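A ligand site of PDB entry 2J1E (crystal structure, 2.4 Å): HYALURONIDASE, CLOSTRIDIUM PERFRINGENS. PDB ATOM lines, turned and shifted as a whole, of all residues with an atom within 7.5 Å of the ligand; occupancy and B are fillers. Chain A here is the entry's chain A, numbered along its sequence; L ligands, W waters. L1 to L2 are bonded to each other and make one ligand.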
ATOM      1  N   GLU A  20      18.452  -3.215   4.296  1.00  0.00           N
ATOM      2  CA  GLU A  20      17.867  -1.946   4.712  1.00  0.00           C
ATOM      3  C   GLU A  20      16.402  -2.087   5.065  1.00  0.00           C
ATOM      4  O   GLU A  20      15.566  -2.490   4.223  1.00  0.00           O
ATOM      5  CB  GLU A  20      17.995  -0.927   3.594  1.00  0.00           C
ATOM      6  CG  GLU A  20      17.529   0.458   3.974  1.00  0.00           C
ATOM      7  CD  GLU A  20      18.323   1.053   5.142  1.00  0.00           C
ATOM      8  OE1 GLU A  20      19.580   1.007   5.097  1.00  0.00           O
ATOM      9  OE2 GLU A  20      17.704   1.588   6.109  1.00  0.00           O
ATOM     10  N   GLY A  23      15.796   3.272   6.351  1.00  0.00           N
ATOM     11  CA  GLY A  23      15.668   4.343   5.376  1.00  0.00           C
ATOM     12  C   GLY A  23      14.643   4.098   4.274  1.00  0.00           C
ATOM     13  O   GLY A  23      14.116   5.039   3.641  1.00  0.00           O
ATOM     14  N   GLU A  24      14.367   2.824   4.010  1.00  0.00           N
ATOM     15  CA  GLU A  24      13.287   2.372   3.091  1.00  0.00           C
ATOM     16  C   GLU A  24      13.102   0.891   3.464  1.00  0.00           C
ATOM     17  O   GLU A  24      13.835   0.366   4.310  1.00  0.00           O
ATOM     18  CB  GLU A  24      13.703   2.539   1.612  1.00  0.00           C
ATOM     19  CG  GLU A  24      14.860   1.594   1.209  1.00  0.00           C
ATOM     20  CD  GLU A  24      15.515   1.987  -0.104  1.00  0.00           C
ATOM     21  OE1 GLU A  24      14.801   2.152  -1.112  1.00  0.00           O
ATOM     22  OE2 GLU A  24      16.745   2.138  -0.124  1.00  0.00           O
ATOM     23  N   ALA A  26      13.692  -2.589   2.296  1.00  0.00           N
ATOM     24  CA  ALA A  26      14.429  -3.389   1.315  1.00  0.00           C
ATOM     25  C   ALA A  26      15.177  -4.592   1.941  1.00  0.00           C
ATOM     26  O   ALA A  26      16.406  -4.761   1.699  1.00  0.00           O
ATOM     27  CB  ALA A  26      15.413  -2.478   0.506  1.00  0.00           C
ATOM     28  N   PHE A  39      12.937  -4.651  -4.096  1.00  0.00           N
ATOM     29  CA  PHE A  39      14.336  -5.115  -4.065  1.00  0.00           C
ATOM     30  C   PHE A  39      14.886  -5.224  -2.666  1.00  0.00           C
ATOM     31  O   PHE A  39      14.401  -4.578  -1.702  1.00  0.00           O
ATOM     32  CB  PHE A  39      15.261  -4.149  -4.865  1.00  0.00           C
ATOM     33  CG  PHE A  39      15.102  -2.717  -4.447  1.00  0.00           C
ATOM     34  CD1 PHE A  39      15.951  -2.165  -3.483  1.00  0.00           C
ATOM     35  CD2 PHE A  39      14.044  -1.947  -4.992  1.00  0.00           C
ATOM     36  CE1 PHE A  39      15.769  -0.844  -3.050  1.00  0.00           C
ATOM     37  CE2 PHE A  39      13.865  -0.642  -4.612  1.00  0.00           C
ATOM     38  CZ  PHE A  39      14.733  -0.074  -3.608  1.00  0.00           C
ATOM     39  N   HIS A  41      18.096  -4.136  -0.566  1.00  0.00           N
ATOM     40  CA  HIS A  41      19.219  -3.226  -0.535  1.00  0.00           C
ATOM     41  C   HIS A  41      20.077  -3.645   0.658  1.00  0.00           C
ATOM     42  O   HIS A  41      19.540  -3.887   1.769  1.00  0.00           O
ATOM     43  CB  HIS A  41      18.734  -1.799  -0.345  1.00  0.00           C
ATOM     44  CG  HIS A  41      19.680  -0.746  -0.869  1.00  0.00           C
ATOM     45  ND1 HIS A  41      20.988  -0.627  -0.437  1.00  0.00           N
ATOM     46  CD2 HIS A  41      19.478   0.291  -1.741  1.00  0.00           C
ATOM     47  CE1 HIS A  41      21.560   0.388  -1.050  1.00  0.00           C
ATOM     48  NE2 HIS A  41      20.667   0.964  -1.856  1.00  0.00           N
ATOM     49  N   SER A  42      21.393  -3.687   0.454  1.00  0.00           N
ATOM     50  CA  SER A  42      22.317  -3.693   1.589  1.00  0.00           C
ATOM     51  C   SER A  42      21.975  -2.500   2.548  1.00  0.00           C
ATOM     52  O   SER A  42      21.412  -1.495   2.087  1.00  0.00           O
ATOM     53  CB  SER A  42      23.768  -3.588   1.099  1.00  0.00           C
ATOM     54  OG  SER A  42      23.949  -2.355   0.372  1.00  0.00           O
ATOM     55  N   TRP A  44      22.205   0.873   4.077  1.00  0.00           N
ATOM     56  CA  TRP A  44      22.874   2.118   3.766  1.00  0.00           C
ATOM     57  C   TRP A  44      22.628   3.211   4.821  1.00  0.00           C
ATOM     58  O   TRP A  44      23.341   4.209   4.865  1.00  0.00           O
ATOM     59  CB  TRP A  44      22.490   2.628   2.400  1.00  0.00           C
ATOM     60  CG  TRP A  44      21.026   2.784   2.158  1.00  0.00           C
ATOM     61  CD1 TRP A  44      20.150   1.845   1.594  1.00  0.00           C
ATOM     62  CD2 TRP A  44      20.242   3.964   2.405  1.00  0.00           C
ATOM     63  NE1 TRP A  44      18.889   2.380   1.506  1.00  0.00           N
ATOM     64  CE2 TRP A  44      18.913   3.677   1.984  1.00  0.00           C
ATOM     65  CE3 TRP A  44      20.516   5.247   2.925  1.00  0.00           C
ATOM     66  CZ2 TRP A  44      17.875   4.616   2.075  1.00  0.00           C
ATOM     67  CZ3 TRP A  44      19.475   6.189   3.025  1.00  0.00           C
ATOM     68  CH2 TRP A  44      18.162   5.848   2.619  1.00  0.00           C
ATOM     69  N   SER A  45      21.604   3.032   5.643  1.00  0.00           N
ATOM     70  CA  SER A  45      21.269   4.031   6.648  1.00  0.00           C
ATOM     71  C   SER A  45      22.246   3.808   7.802  1.00  0.00           C
ATOM     72  O   SER A  45      22.739   2.718   7.984  1.00  0.00           O
ATOM     73  CB  SER A  45      19.808   3.937   7.046  1.00  0.00           C
ATOM     74  OG  SER A  45      19.579   2.717   7.756  1.00  0.00           O
ATOM     75  N   ARG A  73      17.948  -4.150  -9.342  1.00  0.00           N
ATOM     76  CA  ARG A  73      17.038  -3.065  -8.975  1.00  0.00           C
ATOM     77  C   ARG A  73      16.645  -2.272 -10.230  1.00  0.00           C
ATOM     78  O   ARG A  73      17.524  -1.916 -11.058  1.00  0.00           O
ATOM     79  CB  ARG A  73      17.769  -2.146  -7.986  1.00  0.00           C
ATOM     80  CG  ARG A  73      16.929  -1.136  -7.355  1.00  0.00           C
ATOM     81  CD  ARG A  73      17.692  -0.183  -6.467  1.00  0.00           C
ATOM     82  NE  ARG A  73      16.863   0.973  -6.093  1.00  0.00           N
ATOM     83  CZ  ARG A  73      17.142   1.820  -5.139  1.00  0.00           C
ATOM     84  NH1 ARG A  73      18.269   1.678  -4.452  1.00  0.00           N
ATOM     85  NH2 ARG A  73      16.281   2.816  -4.868  1.00  0.00           N
ATOM     86  N   ASP A  75      14.824   0.888 -10.352  1.00  0.00           N
ATOM     87  CA  ASP A  75      14.560   2.328 -10.286  1.00  0.00           C
ATOM     88  C   ASP A  75      15.847   3.123 -10.024  1.00  0.00           C
ATOM     89  O   ASP A  75      15.821   4.327  -9.954  1.00  0.00           O
ATOM     90  CB  ASP A  75      13.509   2.644  -9.199  1.00  0.00           C
ATOM     91  CG  ASP A  75      13.992   2.254  -7.798  1.00  0.00           C
ATOM     92  OD1 ASP A  75      14.658   1.182  -7.685  1.00  0.00           O
ATOM     93  OD2 ASP A  75      13.776   2.956  -6.771  1.00  0.00           O
ATOM     94  N   SER A  76      16.969   2.428  -9.860  1.00  0.00           N
ATOM     95  CA  SER A  76      18.219   3.103  -9.494  1.00  0.00           C
ATOM     96  C   SER A  76      19.358   2.123  -9.742  1.00  0.00           C
ATOM     97  O   SER A  76      19.169   0.919  -9.631  1.00  0.00           O
ATOM     98  CB  SER A  76      18.189   3.493  -8.004  1.00  0.00           C
ATOM     99  OG  SER A  76      19.454   3.808  -7.508  1.00  0.00           O
ATOM    100  N   LYS A  77      20.529   2.665 -10.092  1.00  0.00           N
ATOM    101  CA  LYS A  77      21.727   1.817 -10.260  1.00  0.00           C
ATOM    102  C   LYS A  77      22.510   1.567  -8.974  1.00  0.00           C
ATOM    103  O   LYS A  77      23.476   0.805  -9.010  1.00  0.00           O
ATOM    104  CB  LYS A  77      22.667   2.300 -11.395  1.00  0.00           C
ATOM    105  CG  LYS A  77      23.434   3.580 -11.123  1.00  0.00           C
ATOM    106  CD  LYS A  77      24.241   3.978 -12.370  1.00  0.00           C
ATOM    107  CE  LYS A  77      25.374   2.967 -12.611  1.00  0.00           C
ATOM    108  NZ  LYS A  77      26.163   3.327 -13.877  1.00  0.00           N
ATOM    109  N   ASN A  78      22.088   2.180  -7.860  1.00  0.00           N
ATOM    110  CA  ASN A  78      22.821   2.034  -6.600  1.00  0.00           C
ATOM    111  C   ASN A  78      22.820   0.540  -6.185  1.00  0.00           C
ATOM    112  O   ASN A  78      21.745  -0.067  -6.057  1.00  0.00           O
ATOM    113  CB  ASN A  78      22.161   2.902  -5.533  1.00  0.00           C
ATOM    114  CG  ASN A  78      22.541   4.382  -5.602  1.00  0.00           C
ATOM    115  OD1 ASN A  78      21.930   5.197  -4.927  1.00  0.00           O
ATOM    116  ND2 ASN A  78      23.558   4.716  -6.363  1.00  0.00           N
ATOM    117  N   GLY A  79      23.992  -0.057  -6.028  1.00  0.00           N
ATOM    118  CA  GLY A  79      24.083  -1.453  -5.621  1.00  0.00           C
ATOM    119  C   GLY A  79      24.078  -2.500  -6.752  1.00  0.00           C
ATOM    120  O   GLY A  79      24.218  -3.707  -6.515  1.00  0.00           O
ATOM    121  N   SER A 131      26.952   2.665  -8.744  1.00  0.00           N
ATOM    122  CA  SER A 131      26.117   3.635  -8.015  1.00  0.00           C
ATOM    123  C   SER A 131      25.996   4.902  -8.865  1.00  0.00           C
ATOM    124  O   SER A 131      26.821   5.089  -9.770  1.00  0.00           O
ATOM    125  CB  SER A 131      26.780   3.960  -6.670  1.00  0.00           C
ATOM    126  OG  SER A 131      26.263   5.126  -6.100  1.00  0.00           O
ATOM    127  N   ASP A 132      24.996   5.757  -8.583  1.00  0.00           N
ATOM    128  CA  ASP A 132      24.862   6.996  -9.300  1.00  0.00           C
ATOM    129  C   ASP A 132      25.589   8.115  -8.547  1.00  0.00           C
ATOM    130  O   ASP A 132      25.624   9.249  -9.033  1.00  0.00           O
ATOM    131  CB  ASP A 132      23.400   7.348  -9.620  1.00  0.00           C
ATOM    132  CG  ASP A 132      22.568   7.550  -8.380  1.00  0.00           C
ATOM    133  OD1 ASP A 132      21.341   7.397  -8.534  1.00  0.00           O
ATOM    134  OD2 ASP A 132      23.039   7.881  -7.244  1.00  0.00           O
ATOM    135  N   GLN A 133      26.182   7.752  -7.404  1.00  0.00           N
ATOM    136  CA  GLN A 133      27.004   8.635  -6.591  1.00  0.00           C
ATOM    137  C   GLN A 133      28.474   8.511  -6.981  1.00  0.00           C
ATOM    138  O   GLN A 133      29.007   7.394  -7.218  1.00  0.00           O
ATOM    139  CB  GLN A 133      26.797   8.291  -5.120  1.00  0.00           C
ATOM    140  CG  GLN A 133      25.284   8.326  -4.710  1.00  0.00           C
ATOM    141  CD  GLN A 133      25.047   7.777  -3.337  1.00  0.00           C
ATOM    142  OE1 GLN A 133      26.028   7.453  -2.618  1.00  0.00           O
ATOM    143  NE2 GLN A 133      23.764   7.658  -2.931  1.00  0.00           N
ATOM    144  N   ALA A 134      29.137   9.662  -7.063  1.00  0.00           N
ATOM    145  CA  ALA A 134      30.540   9.738  -7.521  1.00  0.00           C
ATOM    146  C   ALA A 134      31.519   8.858  -6.708  1.00  0.00           C
ATOM    147  O   ALA A 134      32.465   8.238  -7.262  1.00  0.00           O
ATOM    148  CB  ALA A 134      31.011  11.239  -7.574  1.00  0.00           C
ATOM    149  N   LYS A 139      29.826   0.439  -2.433  1.00  0.00           N
ATOM    150  CA  LYS A 139      29.216   0.745  -1.123  1.00  0.00           C
ATOM    151  C   LYS A 139      27.910   0.002  -0.941  1.00  0.00           C
ATOM    152  O   LYS A 139      27.512  -0.288   0.200  1.00  0.00           O
ATOM    153  CB  LYS A 139      28.856   2.229  -0.981  1.00  0.00           C
ATOM    154  CG  LYS A 139      29.933   3.135  -0.525  1.00  0.00           C
ATOM    155  CD  LYS A 139      29.358   4.520  -0.156  1.00  0.00           C
ATOM    156  CE  LYS A 139      30.550   5.447   0.165  1.00  0.00           C
ATOM    157  NZ  LYS A 139      30.271   6.911  -0.186  1.00  0.00           N
ATOM    158  N   PHE A 140      27.217  -0.246  -2.056  1.00  0.00           N
ATOM    159  CA  PHE A 140      25.850  -0.756  -2.044  1.00  0.00           C
ATOM    160  C   PHE A 140      25.694  -2.088  -2.733  1.00  0.00           C
ATOM    161  O   PHE A 140      26.492  -2.449  -3.595  1.00  0.00           O
ATOM    162  CB  PHE A 140      24.876   0.271  -2.669  1.00  0.00           C
ATOM    163  CG  PHE A 140      25.093   1.683  -2.165  1.00  0.00           C
ATOM    164  CD1 PHE A 140      25.402   2.735  -3.070  1.00  0.00           C
ATOM    165  CD2 PHE A 140      24.998   1.964  -0.789  1.00  0.00           C
ATOM    166  CE1 PHE A 140      25.594   4.045  -2.602  1.00  0.00           C
ATOM    167  CE2 PHE A 140      25.211   3.287  -0.303  1.00  0.00           C
ATOM    168  CZ  PHE A 140      25.498   4.316  -1.212  1.00  0.00           C
ATOM    169  N   THR A 142      22.252  -4.234  -4.405  1.00  0.00           N
ATOM    170  CA  THR A 142      20.793  -4.389  -4.527  1.00  0.00           C
ATOM    171  C   THR A 142      20.472  -5.543  -5.516  1.00  0.00           C
ATOM    172  O   THR A 142      21.287  -5.892  -6.397  1.00  0.00           O
ATOM    173  CB  THR A 142      20.160  -3.128  -5.089  1.00  0.00           C
ATOM    174  OG1 THR A 142      20.956  -2.740  -6.231  1.00  0.00           O
ATOM    175  CG2 THR A 142      20.204  -1.942  -4.090  1.00  0.00           C
HETATM  176  C1  LIG L   1      20.337  11.575  -4.802  1.00  0.00           C
HETATM  177  C2  LIG L   1      21.440  10.533  -5.059  1.00  0.00           C
HETATM  178  C3  LIG L   1      20.941   9.057  -5.005  1.00  0.00           C
HETATM  179  C4  LIG L   1      20.060   8.764  -3.787  1.00  0.00           C
HETATM  180  C5  LIG L   1      19.030   9.900  -3.570  1.00  0.00           C
HETATM  181  C6  LIG L   1      18.549   9.856  -2.120  1.00  0.00           C
HETATM  182  C7  LIG L   1      23.287  11.323  -6.378  1.00  0.00           C
HETATM  183  C8  LIG L   1      23.853  11.703  -7.721  1.00  0.00           C
HETATM  184  O1  LIG L   1      19.536  11.221  -3.685  1.00  0.00           O
HETATM  185  O2  LIG L   1      22.001   8.130  -4.912  1.00  0.00           O
HETATM  186  O3  LIG L   1      19.413   7.478  -3.899  1.00  0.00           O
HETATM  187  O4  LIG L   1      17.156   9.957  -2.295  1.00  0.00           O
HETATM  188  O5  LIG L   1      23.945  11.438  -5.341  1.00  0.00           O
HETATM  189  N1  LIG L   1      22.048  10.863  -6.328  1.00  0.00           N
HETATM  190  O6  LIG L   1      19.450  11.619  -5.906  1.00  0.00           O
HETATM  191  C1  LG2 L   2      19.377   6.734  -2.685  1.00  0.00           C
HETATM  192  C2  LG2 L   2      18.411   5.568  -2.970  1.00  0.00           C
HETATM  193  C3  LG2 L   2      18.451   4.517  -1.871  1.00  0.00           C
HETATM  194  C4  LG2 L   2      19.906   4.123  -1.552  1.00  0.00           C
HETATM  195  C5  LG2 L   2      20.702   5.416  -1.199  1.00  0.00           C
HETATM  196  C6  LG2 L   2      22.148   5.156  -0.812  1.00  0.00           C
HETATM  197  O1  LG2 L   2      17.077   6.028  -3.212  1.00  0.00           O
HETATM  198  O2  LG2 L   2      17.674   3.391  -2.271  1.00  0.00           O
HETATM  199  O3  LG2 L   2      20.470   3.427  -2.646  1.00  0.00           O
HETATM  200  O4  LG2 L   2      20.678   6.326  -2.265  1.00  0.00           O
HETATM  201  O5  LG2 L   2      22.788   6.388  -0.556  1.00  0.00           O
HETATM  202  O   HOH W   1      24.573   6.205   1.516  1.00  0.00           O
HETATM  203  O   HOH W   2      17.543  10.568  -7.985  1.00  0.00           O
HETATM  204  O   HOH W   3      20.135  12.822  -1.028  1.00  0.00           O
HETATM  205  O   HOH W   4      14.653   4.561  -2.637  1.00  0.00           O
HETATM  206  O   HOH W   5      15.437  11.464  -0.419  1.00  0.00           O
HETATM  207  O   HOH W   6      19.566   6.348  -6.665  1.00  0.00           O
HETATM  208  O   HOH W   7      20.242  10.128  -8.450  1.00  0.00           O
HETATM  209  O   HOH W   8      16.150   6.852  -5.583  1.00  0.00           O
HETATM  210  O   HOH W   9      21.092   8.731  -0.133  1.00  0.00           O
HETATM  211  O   HOH W  10      17.430  13.689  -5.501  1.00  0.00           O
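Water W7 bridges a nitrogen (N1) of LIG L1 and the side-chain carboxylate (OD1) of Asp 132.
Water W4 lies within hydrogen-bond range of the side-chain carboxylate (OE1) of Glu 24 (2.9 Å), an oxygen (O1) of LG2 L2 (2.9 Å) and the guanidinium group (NH2) of Arg 73 (3.3 Å).
The side-chain amide nitrogen (NE2) of Gln 133 sits at hydrogen-bond distance from an oxygen (O2) of LIG L1 (2.7 Å).
The guanidinium group (NH1) of Arg 73 lies within hydrogen-bond range of an oxygen (O2) of LG2 L2 (2.8 Å).
The side-chain carboxylate of Asp 132 sits at hydrogen-bond distance from an oxygen (O2) of LIG L1 (2.6 Å).
The side-chain amide oxygen of Asn 78 sits at hydrogen-bond distance from an oxygen (O2) of LIG L1.
O3 of LG2 L2 is in hydrogen-bond range of NE2 of His 41 (2.6 Å).
The side-chain carboxylate (OE2) of Glu 24 is in hydrogen-bond range of an oxygen (O2) of LG2 L2 (2.7 Å).
O of Asn 78 is in hydrogen-bond range of OG1 of Thr 142, at 2.8 Å.
The backbone NH (N) of Glu 20 is in hydrogen-bond range of the backbone carbonyl oxygen (O) of His 41 (2.8 Å).
N of Gln 133 is in hydrogen-bond range of OG of Ser 131 (2.9 Å).
OE2 of Glu 24 lies within hydrogen-bond range of NE1 of Trp 44 (2.7 Å).
ND2 of Asn 78 is in hydrogen-bond range of OG of Ser 131, at 2.7 Å.
N of Asn 78 is in hydrogen-bond range of OG of Ser 76, 3.1 Å away.
N of Asp 132 sits close to ND2 of Asn 78 (2.8 Å).
O of Ala 26 sits at hydrogen-bond distance from N of His 41 (2.9 Å).
NE1 of Trp 44 touches C4 of LG2 L2, at 3.7 Å.
Phe 140 touches the ligand.
The nearest printed residue that does not touch the ligand is Phe 39 (4.7 Å).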
